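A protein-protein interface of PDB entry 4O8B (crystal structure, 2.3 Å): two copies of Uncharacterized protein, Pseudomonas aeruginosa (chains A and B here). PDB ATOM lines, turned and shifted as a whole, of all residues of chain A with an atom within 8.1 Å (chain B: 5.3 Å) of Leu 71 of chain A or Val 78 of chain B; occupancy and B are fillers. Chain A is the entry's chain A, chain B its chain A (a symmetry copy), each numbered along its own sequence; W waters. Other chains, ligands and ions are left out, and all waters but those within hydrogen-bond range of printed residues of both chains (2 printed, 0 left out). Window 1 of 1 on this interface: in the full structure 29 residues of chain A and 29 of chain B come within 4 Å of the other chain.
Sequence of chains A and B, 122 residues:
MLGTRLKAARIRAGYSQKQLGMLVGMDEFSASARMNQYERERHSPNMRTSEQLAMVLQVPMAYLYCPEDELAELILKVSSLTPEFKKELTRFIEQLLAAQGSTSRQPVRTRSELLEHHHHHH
Of the 21 printed residues of chain A, 10 touch a printed residue of chain B. Hydrophobic or aromatic side chains of chain A that line the printed part of chain B: Ala 62, Leu 71, Leu 74, Ile 75, Leu 89, Ile 93 and Leu 97. Among the printed residues, 19 pairs touch across the chains.
Printed residues of chain B within 4 Å of Leu 71 of chain A: Pro 60, Ile 75, Val 78 and Ser 79. Printed residues of chain A within 4 Å of Val 78 of chain B: Leu 71. Printed residues of chain A within 4 Å of Ala 62 of chain B: Ala 62 (3.6 Å), Tyr 65 (3.3 Å), Cys 66 (3.9 Å) and Ile 75 (3.97 Å). Printed residues of chain A within 4 Å of Lys 77 of chain B: Leu 97. Arg 5 of chain A touches none of the printed residues of chain B. Lys 77 of chain A touches none of the printed residues of chain B. The nearest residue of chain B that does not touch Leu 71 of chain A is Ala 62 of chain B (5.0 Å). The nearest residue of chain A that does not touch Val 78 of chain B is Leu 74 of chain A (4.2 Å).
Ala 62 of chain A touches its own counterpart, Ala 62 of chain B. Ala 62 of chain A touches Ile 75 of chain B, and with the chains exchanged Ile 75 of chain A touches Ala 62 of chain B. Leu 74 of chain A touches Leu 89 of chain B, and with the chains exchanged Leu 89 of chain A touches Leu 74 of chain B. Ile 75 of chain B touches its own counterpart, Ile 75 of chain A. Of the 19 pairs that touch across the chains among the printed residues, 6 have their exchanged pair printed and touching as well.
N of Ala 62 of chain B lies within hydrogen-bond range of O of Tyr 65 of chain A. The backbone carbonyl oxygen (O) of Ser 80 of chain B sits close to the backbone carbonyl oxygen (O) of Gly 101 of chain A, 3.5 Å away.
Ala 62 of chain A touches Ala 62 of chain B. CD1 of Ile 75 of chain B touches CB of Ala 62 of chain A, 3.97 Å away. Cys 66 of chain A touches Ala 62 of chain B. Pro 60 of chain B touches Leu 71 of chain A (CB to CD2, 3.7 Å). CD2 of Leu 71 of chain A touches OG of Ser 79 of chain B (3.7 Å). Leu 74 of chain A touches Leu 89 of chain B. Ile 75 of chain A touches Ala 62 of chain B (CD1 to CB, 3.97 Å). CD1 of Ile 93 of chain A touches CD1 of Leu 74 of chain B, 3.7 Å away. CG of Lys 77 of chain B touches CD1 of Leu 97 of chain A (3.6 Å). Leu 81 of chain B touches Gly 101 of chain A (CD2 to O, 3.1 Å).
Water W1 lies within hydrogen-bond range of OE1 of Glu 68 of chain A, N of Ala 62 of chain B and SG of Cys 66 of chain A. Water W2 lies within hydrogen-bond range of the backbone carbonyl oxygen of Lys 86 of chain B (3.3 Å) and the side-chain carboxylate of Glu 70 of chain A (3.3 Å).
NE of Arg 5 of chain A lies within hydrogen-bond range of O of Cys 66 of chain A (2.7 Å). The backbone carbonyl oxygen (O) of Glu 68 of chain A lies within hydrogen-bond range of the side-chain sulfur (SG) of Cys 66 of chain A (3.1 Å). The side-chain sulfur of Cys 66 of chain A lies within hydrogen-bond range of the backbone NH of Ala 72 of chain A, 2.9 Å away. OG of Ser 79 of chain B lies within hydrogen-bond range of O of Ile 75 of chain B (2.8 Å). The backbone carbonyl oxygen (O) of Leu 76 of chain B is in hydrogen-bond range of the side-chain hydroxyl (OG) of Ser 80 of chain B (2.9 Å). The backbone carbonyl oxygen (O) of Lys 77 of chain B lies within hydrogen-bond range of the side-chain hydroxyl (OG) of Ser 80 of chain B, at 2.6 Å.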
ATOM      1  N   ARG A   5     -13.733 -14.507  11.084  1.00  0.00           N
ATOM      2  CA  ARG A   5     -14.847 -15.446  10.927  1.00  0.00           C
ATOM      3  C   ARG A   5     -15.564 -15.657  12.255  1.00  0.00           C
ATOM      4  O   ARG A   5     -16.789 -15.742  12.300  1.00  0.00           O
ATOM      5  CB  ARG A   5     -14.327 -16.786  10.407  1.00  0.00           C
ATOM      6  CG  ARG A   5     -13.531 -16.678   9.110  1.00  0.00           C
ATOM      7  CD  ARG A   5     -14.429 -16.369   7.923  1.00  0.00           C
ATOM      8  NE  ARG A   5     -13.649 -16.080   6.721  1.00  0.00           N
ATOM      9  CZ  ARG A   5     -13.561 -14.876   6.156  1.00  0.00           C
ATOM     10  NH1 ARG A   5     -14.199 -13.842   6.690  1.00  0.00           N
ATOM     11  NH2 ARG A   5     -12.809 -14.707   5.077  1.00  0.00           N
ATOM     12  N   ALA A  62     -16.202 -25.349   9.350  1.00  0.00           N
ATOM     13  CA  ALA A  62     -15.384 -24.985   8.202  1.00  0.00           C
ATOM     14  C   ALA A  62     -15.340 -23.472   7.988  1.00  0.00           C
ATOM     15  O   ALA A  62     -14.295 -22.921   7.650  1.00  0.00           O
ATOM     16  CB  ALA A  62     -15.923 -25.670   6.949  1.00  0.00           C
ATOM     17  N   TYR A  63     -16.479 -22.814   8.183  1.00  0.00           N
ATOM     18  CA  TYR A  63     -16.565 -21.373   8.011  1.00  0.00           C
ATOM     19  C   TYR A  63     -15.511 -20.651   8.851  1.00  0.00           C
ATOM     20  O   TYR A  63     -14.820 -19.751   8.362  1.00  0.00           O
ATOM     21  CB  TYR A  63     -17.953 -20.871   8.409  1.00  0.00           C
ATOM     22  CG  TYR A  63     -18.086 -19.366   8.394  1.00  0.00           C
ATOM     23  CD1 TYR A  63     -18.024 -18.655   7.196  1.00  0.00           C
ATOM     24  CD2 TYR A  63     -18.208 -18.643   9.585  1.00  0.00           C
ATOM     25  CE1 TYR A  63     -18.124 -17.259   7.178  1.00  0.00           C
ATOM     26  CE2 TYR A  63     -18.309 -17.253   9.580  1.00  0.00           C
ATOM     27  CZ  TYR A  63     -18.245 -16.569   8.375  1.00  0.00           C
ATOM     28  OH  TYR A  63     -18.333 -15.199   8.361  1.00  0.00           O
ATOM     29  N   TYR A  65     -12.825 -21.575   9.635  1.00  0.00           N
ATOM     30  CA  TYR A  65     -11.495 -21.919   9.128  1.00  0.00           C
ATOM     31  C   TYR A  65     -11.415 -21.679   7.624  1.00  0.00           C
ATOM     32  O   TYR A  65     -10.619 -22.311   6.929  1.00  0.00           O
ATOM     33  CB  TYR A  65     -11.178 -23.387   9.427  1.00  0.00           C
ATOM     34  CG  TYR A  65     -10.796 -23.666  10.862  1.00  0.00           C
ATOM     35  CD1 TYR A  65      -9.508 -23.389  11.331  1.00  0.00           C
ATOM     36  CD2 TYR A  65     -11.726 -24.195  11.761  1.00  0.00           C
ATOM     37  CE1 TYR A  65      -9.151 -23.650  12.650  1.00  0.00           C
ATOM     38  CE2 TYR A  65     -11.376 -24.454  13.090  1.00  0.00           C
ATOM     39  CZ  TYR A  65     -10.092 -24.173  13.525  1.00  0.00           C
ATOM     40  OH  TYR A  65      -9.751 -24.428  14.834  1.00  0.00           O
ATOM     41  N   CYS A  66     -12.241 -20.764   7.127  1.00  0.00           N
ATOM     42  CA  CYS A  66     -12.268 -20.436   5.703  1.00  0.00           C
ATOM     43  C   CYS A  66     -11.669 -19.061   5.429  1.00  0.00           C
ATOM     44  O   CYS A  66     -12.371 -18.054   5.461  1.00  0.00           O
ATOM     45  CB  CYS A  66     -13.706 -20.488   5.186  1.00  0.00           C
ATOM     46  SG  CYS A  66     -13.904 -19.835   3.517  1.00  0.00           S
ATOM     47  N   PRO A  67     -10.362 -19.000   5.156  1.00  0.00           N
ATOM     48  CA  PRO A  67      -9.690 -17.723   4.881  1.00  0.00           C
ATOM     49  C   PRO A  67     -10.162 -17.037   3.595  1.00  0.00           C
ATOM     50  O   PRO A  67     -10.117 -15.812   3.493  1.00  0.00           O
ATOM     51  CB  PRO A  67      -8.212 -18.106   4.837  1.00  0.00           C
ATOM     52  CG  PRO A  67      -8.252 -19.506   4.318  1.00  0.00           C
ATOM     53  CD  PRO A  67      -9.392 -20.112   5.106  1.00  0.00           C
ATOM     54  N   GLU A  68     -10.603 -17.824   2.616  1.00  0.00           N
ATOM     55  CA  GLU A  68     -11.083 -17.265   1.362  1.00  0.00           C
ATOM     56  C   GLU A  68     -12.443 -16.619   1.572  1.00  0.00           C
ATOM     57  O   GLU A  68     -13.440 -17.306   1.775  1.00  0.00           O
ATOM     58  CB  GLU A  68     -11.191 -18.346   0.286  1.00  0.00           C
ATOM     59  CG  GLU A  68      -9.863 -18.851  -0.273  1.00  0.00           C
ATOM     60  CD  GLU A  68      -9.225 -19.910   0.602  1.00  0.00           C
ATOM     61  OE1 GLU A  68      -9.971 -20.748   1.159  1.00  0.00           O
ATOM     62  OE2 GLU A  68      -7.977 -19.936   0.706  1.00  0.00           O
ATOM     63  N   ASP A  69     -12.485 -15.290   1.520  1.00  0.00           N
ATOM     64  CA  ASP A  69     -13.736 -14.552   1.729  1.00  0.00           C
ATOM     65  C   ASP A  69     -14.896 -15.029   0.860  1.00  0.00           C
ATOM     66  O   ASP A  69     -16.011 -15.188   1.355  1.00  0.00           O
ATOM     67  CB  ASP A  69     -13.507 -13.057   1.510  1.00  0.00           C
ATOM     68  CG  ASP A  69     -12.537 -12.453   2.513  1.00  0.00           C
ATOM     69  OD1 ASP A  69     -12.864 -12.421   3.720  1.00  0.00           O
ATOM     70  OD2 ASP A  69     -11.435 -12.028   2.097  1.00  0.00           O
ATOM     71  N   GLU A  70     -14.650 -15.257  -0.426  1.00  0.00           N
ATOM     72  CA  GLU A  70     -15.718 -15.709  -1.316  1.00  0.00           C
ATOM     73  C   GLU A  70     -16.296 -17.060  -0.908  1.00  0.00           C
ATOM     74  O   GLU A  70     -17.512 -17.220  -0.827  1.00  0.00           O
ATOM     75  CB  GLU A  70     -15.226 -15.802  -2.769  1.00  0.00           C
ATOM     76  CG  GLU A  70     -15.412 -14.529  -3.581  1.00  0.00           C
ATOM     77  CD  GLU A  70     -15.506 -14.816  -5.071  1.00  0.00           C
ATOM     78  OE1 GLU A  70     -16.396 -15.612  -5.469  1.00  0.00           O
ATOM     79  OE2 GLU A  70     -14.704 -14.249  -5.845  1.00  0.00           O
ATOM     80  N   LEU A  71     -15.420 -18.025  -0.656  1.00  0.00           N
ATOM     81  CA  LEU A  71     -15.860 -19.361  -0.269  1.00  0.00           C
ATOM     82  C   LEU A  71     -16.650 -19.346   1.036  1.00  0.00           C
ATOM     83  O   LEU A  71     -17.732 -19.932   1.124  1.00  0.00           O
ATOM     84  CB  LEU A  71     -14.654 -20.300  -0.130  1.00  0.00           C
ATOM     85  CG  LEU A  71     -15.002 -21.784  -0.015  1.00  0.00           C
ATOM     86  CD1 LEU A  71     -15.912 -22.182  -1.168  1.00  0.00           C
ATOM     87  CD2 LEU A  71     -13.732 -22.617  -0.031  1.00  0.00           C
ATOM     88  N   ALA A  72     -16.105 -18.679   2.044  1.00  0.00           N
ATOM     89  CA  ALA A  72     -16.767 -18.587   3.344  1.00  0.00           C
ATOM     90  C   ALA A  72     -18.207 -18.132   3.167  1.00  0.00           C
ATOM     91  O   ALA A  72     -19.137 -18.767   3.677  1.00  0.00           O
ATOM     92  CB  ALA A  72     -16.019 -17.602   4.241  1.00  0.00           C
ATOM     93  N   GLU A  73     -18.383 -17.036   2.438  1.00  0.00           N
ATOM     94  CA  GLU A  73     -19.713 -16.497   2.192  1.00  0.00           C
ATOM     95  C   GLU A  73     -20.610 -17.569   1.587  1.00  0.00           C
ATOM     96  O   GLU A  73     -21.793 -17.652   1.905  1.00  0.00           O
ATOM     97  CB  GLU A  73     -19.608 -15.295   1.241  1.00  0.00           C
ATOM     98  CG  GLU A  73     -20.780 -14.331   1.332  1.00  0.00           C
ATOM     99  CD  GLU A  73     -21.106 -13.963   2.770  1.00  0.00           C
ATOM    100  OE1 GLU A  73     -20.180 -13.588   3.520  1.00  0.00           O
ATOM    101  OE2 GLU A  73     -22.299 -14.049   3.150  1.00  0.00           O
ATOM    102  N   LEU A  74     -20.029 -18.396   0.717  1.00  0.00           N
ATOM    103  CA  LEU A  74     -20.778 -19.466   0.062  1.00  0.00           C
ATOM    104  C   LEU A  74     -21.080 -20.596   1.045  1.00  0.00           C
ATOM    105  O   LEU A  74     -22.148 -21.208   0.989  1.00  0.00           O
ATOM    106  CB  LEU A  74     -19.982 -20.015  -1.125  1.00  0.00           C
ATOM    107  CG  LEU A  74     -20.784 -20.310  -2.392  1.00  0.00           C
ATOM    108  CD1 LEU A  74     -21.209 -18.994  -3.035  1.00  0.00           C
ATOM    109  CD2 LEU A  74     -19.943 -21.118  -3.367  1.00  0.00           C
ATOM    110  N   ILE A  75     -20.136 -20.863   1.941  1.00  0.00           N
ATOM    111  CA  ILE A  75     -20.294 -21.926   2.932  1.00  0.00           C
ATOM    112  C   ILE A  75     -21.453 -21.635   3.892  1.00  0.00           C
ATOM    113  O   ILE A  75     -22.086 -22.562   4.403  1.00  0.00           O
ATOM    114  CB  ILE A  75     -19.007 -22.127   3.767  1.00  0.00           C
ATOM    115  CG1 ILE A  75     -17.869 -22.578   2.854  1.00  0.00           C
ATOM    116  CG2 ILE A  75     -19.249 -23.148   4.867  1.00  0.00           C
ATOM    117  CD1 ILE A  75     -16.611 -22.994   3.601  1.00  0.00           C
ATOM    118  N   LEU A  76     -21.713 -20.360   4.134  1.00  0.00           N
ATOM    119  CA  LEU A  76     -22.800 -19.969   5.022  1.00  0.00           C
ATOM    120  C   LEU A  76     -24.125 -20.014   4.284  1.00  0.00           C
ATOM    121  O   LEU A  76     -25.160 -20.360   4.854  1.00  0.00           O
ATOM    122  CB  LEU A  76     -22.567 -18.560   5.580  1.00  0.00           C
ATOM    123  CG  LEU A  76     -21.398 -18.378   6.550  1.00  0.00           C
ATOM    124  CD1 LEU A  76     -21.489 -16.996   7.181  1.00  0.00           C
ATOM    125  CD2 LEU A  76     -21.452 -19.453   7.633  1.00  0.00           C
ATOM    126  N   LYS A  77     -24.082 -19.661   3.004  1.00  0.00           N
ATOM    127  CA  LYS A  77     -25.283 -19.659   2.176  1.00  0.00           C
ATOM    128  C   LYS A  77     -25.799 -21.073   1.936  1.00  0.00           C
ATOM    129  O   LYS A  77     -26.964 -21.365   2.193  1.00  0.00           O
ATOM    130  CB  LYS A  77     -25.004 -18.970   0.838  1.00  0.00           C
ATOM    131  CG  LYS A  77     -24.744 -17.480   0.963  1.00  0.00           C
ATOM    132  CD  LYS A  77     -24.583 -16.834  -0.399  1.00  0.00           C
ATOM    133  CE  LYS A  77     -23.869 -15.496  -0.281  1.00  0.00           C
ATOM    134  NZ  LYS A  77     -23.403 -14.999  -1.613  1.00  0.00           N
ATOM    135  N   VAL A  78     -24.932 -21.943   1.449  1.00  0.00           N
ATOM    136  CA  VAL A  78     -25.314 -23.324   1.172  1.00  0.00           C
ATOM    137  C   VAL A  78     -25.810 -24.022   2.435  1.00  0.00           C
ATOM    138  O   VAL A  78     -26.692 -24.883   2.369  1.00  0.00           O
ATOM    139  CB  VAL A  78     -24.134 -24.127   0.578  1.00  0.00           C
ATOM    140  CG1 VAL A  78     -23.613 -23.434  -0.670  1.00  0.00           C
ATOM    141  CG2 VAL A  78     -23.027 -24.270   1.604  1.00  0.00           C
ATOM    142  N   LEU A  89     -29.120 -27.550  -5.527  1.00  0.00           N
ATOM    143  CA  LEU A  89     -27.787 -26.984  -5.609  1.00  0.00           C
ATOM    144  C   LEU A  89     -26.809 -28.005  -6.193  1.00  0.00           C
ATOM    145  O   LEU A  89     -26.208 -27.769  -7.244  1.00  0.00           O
ATOM    146  CB  LEU A  89     -27.314 -26.549  -4.224  1.00  0.00           C
ATOM    147  CG  LEU A  89     -25.976 -25.799  -4.161  1.00  0.00           C
ATOM    148  CD1 LEU A  89     -26.144 -24.397  -4.721  1.00  0.00           C
ATOM    149  CD2 LEU A  89     -25.497 -25.742  -2.718  1.00  0.00           C
ATOM    150  N   ILE A  93     -24.519 -27.815  -9.538  1.00  0.00           N
ATOM    151  CA  ILE A  93     -23.059 -27.842  -9.471  1.00  0.00           C
ATOM    152  C   ILE A  93     -22.500 -29.002 -10.295  1.00  0.00           C
ATOM    153  O   ILE A  93     -21.559 -28.824 -11.070  1.00  0.00           O
ATOM    154  CB  ILE A  93     -22.570 -27.980  -8.018  1.00  0.00           C
ATOM    155  CG1 ILE A  93     -23.126 -26.828  -7.176  1.00  0.00           C
ATOM    156  CG2 ILE A  93     -21.044 -27.963  -7.976  1.00  0.00           C
ATOM    157  CD1 ILE A  93     -22.838 -26.948  -5.693  1.00  0.00           C
ATOM    158  N   LEU A  97     -19.744 -28.854 -13.233  1.00  0.00           N
ATOM    159  CA  LEU A  97     -18.491 -29.598 -13.175  1.00  0.00           C
ATOM    160  C   LEU A  97     -18.401 -30.527 -14.377  1.00  0.00           C
ATOM    161  O   LEU A  97     -17.315 -30.923 -14.789  1.00  0.00           O
ATOM    162  CB  LEU A  97     -18.423 -30.449 -11.898  1.00  0.00           C
ATOM    163  CG  LEU A  97     -18.257 -29.757 -10.541  1.00  0.00           C
ATOM    164  CD1 LEU A  97     -18.301 -30.808  -9.452  1.00  0.00           C
ATOM    165  CD2 LEU A  97     -16.941 -28.987 -10.487  1.00  0.00           C
ATOM    166  N   GLY A 101     -15.207 -27.051 -15.538  1.00  0.00           N
ATOM    167  CA  GLY A 101     -14.408 -25.838 -15.482  1.00  0.00           C
ATOM    168  C   GLY A 101     -14.601 -25.108 -14.169  1.00  0.00           C
ATOM    169  O   GLY A 101     -15.422 -25.512 -13.334  1.00  0.00           O
ATOM    170  N   PRO B  60      -9.000 -26.193  -0.089  1.00  0.00           N
ATOM    171  CA  PRO B  60      -9.314 -25.110   0.849  1.00  0.00           C
ATOM    172  C   PRO B  60      -9.103 -25.562   2.289  1.00  0.00           C
ATOM    173  O   PRO B  60      -9.498 -26.663   2.661  1.00  0.00           O
ATOM    174  CB  PRO B  60     -10.780 -24.814   0.549  1.00  0.00           C
ATOM    175  CG  PRO B  60     -10.896 -25.146  -0.900  1.00  0.00           C
ATOM    176  CD  PRO B  60     -10.133 -26.442  -0.993  1.00  0.00           C
ATOM    177  N   ALA B  62     -10.626 -24.829   4.760  1.00  0.00           N
ATOM    178  CA  ALA B  62     -11.933 -25.142   5.319  1.00  0.00           C
ATOM    179  C   ALA B  62     -12.280 -26.623   5.169  1.00  0.00           C
ATOM    180  O   ALA B  62     -12.852 -27.224   6.076  1.00  0.00           O
ATOM    181  CB  ALA B  62     -13.001 -24.289   4.640  1.00  0.00           C
ATOM    182  N   LEU B  74     -18.956 -30.511  -1.229  1.00  0.00           N
ATOM    183  CA  LEU B  74     -19.366 -29.320  -1.968  1.00  0.00           C
ATOM    184  C   LEU B  74     -18.252 -28.275  -1.974  1.00  0.00           C
ATOM    185  O   LEU B  74     -18.056 -27.572  -2.966  1.00  0.00           O
ATOM    186  CB  LEU B  74     -20.629 -28.722  -1.344  1.00  0.00           C
ATOM    187  CG  LEU B  74     -21.696 -28.232  -2.323  1.00  0.00           C
ATOM    188  CD1 LEU B  74     -22.357 -29.434  -2.988  1.00  0.00           C
ATOM    189  CD2 LEU B  74     -22.738 -27.403  -1.590  1.00  0.00           C
ATOM    190  N   ILE B  75     -17.528 -28.182  -0.864  1.00  0.00           N
ATOM    191  CA  ILE B  75     -16.438 -27.216  -0.734  1.00  0.00           C
ATOM    192  C   ILE B  75     -15.307 -27.505  -1.728  1.00  0.00           C
ATOM    193  O   ILE B  75     -14.610 -26.584  -2.162  1.00  0.00           O
ATOM    194  CB  ILE B  75     -15.844 -27.212   0.695  1.00  0.00           C
ATOM    195  CG1 ILE B  75     -16.910 -26.769   1.693  1.00  0.00           C
ATOM    196  CG2 ILE B  75     -14.634 -26.292   0.757  1.00  0.00           C
ATOM    197  CD1 ILE B  75     -16.377 -26.540   3.099  1.00  0.00           C
ATOM    198  N   LEU B  76     -15.130 -28.771  -2.070  1.00  0.00           N
ATOM    199  CA  LEU B  76     -14.092 -29.157  -3.016  1.00  0.00           C
ATOM    200  C   LEU B  76     -14.564 -28.924  -4.440  1.00  0.00           C
ATOM    201  O   LEU B  76     -13.784 -28.551  -5.316  1.00  0.00           O
ATOM    202  CB  LEU B  76     -13.710 -30.630  -2.834  1.00  0.00           C
ATOM    203  CG  LEU B  76     -12.992 -31.009  -1.537  1.00  0.00           C
ATOM    204  CD1 LEU B  76     -12.475 -32.436  -1.655  1.00  0.00           C
ATOM    205  CD2 LEU B  76     -11.832 -30.051  -1.287  1.00  0.00           C
ATOM    206  N   LYS B  77     -15.855 -29.146  -4.661  1.00  0.00           N
ATOM    207  CA  LYS B  77     -16.442 -28.962  -5.984  1.00  0.00           C
ATOM    208  C   LYS B  77     -16.460 -27.492  -6.386  1.00  0.00           C
ATOM    209  O   LYS B  77     -15.967 -27.129  -7.451  1.00  0.00           O
ATOM    210  CB  LYS B  77     -17.863 -29.531  -6.018  1.00  0.00           C
ATOM    211  CG  LYS B  77     -17.915 -31.043  -5.894  1.00  0.00           C
ATOM    212  CD  LYS B  77     -19.333 -31.557  -6.044  1.00  0.00           C
ATOM    213  CE  LYS B  77     -19.465 -32.957  -5.462  1.00  0.00           C
ATOM    214  NZ  LYS B  77     -20.897 -33.352  -5.292  1.00  0.00           N
ATOM    215  N   VAL B  78     -17.025 -26.653  -5.535  1.00  0.00           N
ATOM    216  CA  VAL B  78     -17.107 -25.224  -5.816  1.00  0.00           C
ATOM    217  C   VAL B  78     -15.719 -24.619  -6.007  1.00  0.00           C
ATOM    218  O   VAL B  78     -15.546 -23.684  -6.794  1.00  0.00           O
ATOM    219  CB  VAL B  78     -17.840 -24.467  -4.685  1.00  0.00           C
ATOM    220  CG1 VAL B  78     -19.217 -25.071  -4.467  1.00  0.00           C
ATOM    221  CG2 VAL B  78     -17.030 -24.525  -3.405  1.00  0.00           C
ATOM    222  N   SER B  79     -14.733 -25.150  -5.296  1.00  0.00           N
ATOM    223  CA  SER B  79     -13.364 -24.654  -5.399  1.00  0.00           C
ATOM    224  C   SER B  79     -12.737 -25.015  -6.742  1.00  0.00           C
ATOM    225  O   SER B  79     -11.922 -24.262  -7.277  1.00  0.00           O
ATOM    226  CB  SER B  79     -12.497 -25.230  -4.272  1.00  0.00           C
ATOM    227  OG  SER B  79     -12.835 -24.658  -3.026  1.00  0.00           O
ATOM    228  N   SER B  80     -13.116 -26.161  -7.279  1.00  0.00           N
ATOM    229  CA  SER B  80     -12.596 -26.621  -8.563  1.00  0.00           C
ATOM    230  C   SER B  80     -13.292 -25.958  -9.745  1.00  0.00           C
ATOM    231  O   SER B  80     -13.076 -26.343 -10.894  1.00  0.00           O
ATOM    232  CB  SER B  80     -12.732 -28.142  -8.671  1.00  0.00           C
ATOM    233  OG  SER B  80     -14.011 -28.575  -8.241  1.00  0.00           O
ATOM    234  N   LEU B  81     -14.122 -24.961  -9.461  1.00  0.00           N
ATOM    235  CA  LEU B  81     -14.844 -24.255 -10.510  1.00  0.00           C
ATOM    236  C   LEU B  81     -14.044 -23.078 -11.059  1.00  0.00           C
ATOM    237  O   LEU B  81     -13.336 -22.395 -10.320  1.00  0.00           O
ATOM    238  CB  LEU B  81     -16.194 -23.748  -9.995  1.00  0.00           C
ATOM    239  CG  LEU B  81     -17.320 -24.769  -9.780  1.00  0.00           C
ATOM    240  CD1 LEU B  81     -18.586 -24.027  -9.364  1.00  0.00           C
ATOM    241  CD2 LEU B  81     -17.562 -25.549 -11.059  1.00  0.00           C
ATOM    242  N   LYS B  86     -17.888 -20.047 -11.410  1.00  0.00           N
ATOM    243  CA  LYS B  86     -18.063 -19.644 -10.023  1.00  0.00           C
ATOM    244  C   LYS B  86     -19.100 -18.525  -9.924  1.00  0.00           C
ATOM    245  O   LYS B  86     -19.811 -18.406  -8.927  1.00  0.00           O
ATOM    246  CB  LYS B  86     -16.715 -19.189  -9.445  1.00  0.00           C
ATOM    247  CG  LYS B  86     -16.561 -19.415  -7.953  1.00  0.00           C
ATOM    248  CD  LYS B  86     -15.104 -19.287  -7.511  1.00  0.00           C
ATOM    249  CE  LYS B  86     -14.367 -20.618  -7.611  1.00  0.00           C
ATOM    250  NZ  LYS B  86     -12.977 -20.548  -7.066  1.00  0.00           N
ATOM    251  N   LEU B  89     -22.596 -20.026 -10.297  1.00  0.00           N
ATOM    252  CA  LEU B  89     -22.973 -20.692  -9.065  1.00  0.00           C
ATOM    253  C   LEU B  89     -23.640 -19.703  -8.106  1.00  0.00           C
ATOM    254  O   LEU B  89     -24.800 -19.881  -7.729  1.00  0.00           O
ATOM    255  CB  LEU B  89     -21.742 -21.305  -8.401  1.00  0.00           C
ATOM    256  CG  LEU B  89     -21.993 -22.168  -7.157  1.00  0.00           C
ATOM    257  CD1 LEU B  89     -22.629 -23.487  -7.564  1.00  0.00           C
ATOM    258  CD2 LEU B  89     -20.675 -22.414  -6.438  1.00  0.00           C
HETATM  259  O   HOH W   1     -11.198 -22.265   2.876  1.00  0.00           O
HETATM  260  O   HOH W   2     -18.759 -15.445  -7.818  1.00  0.00           O
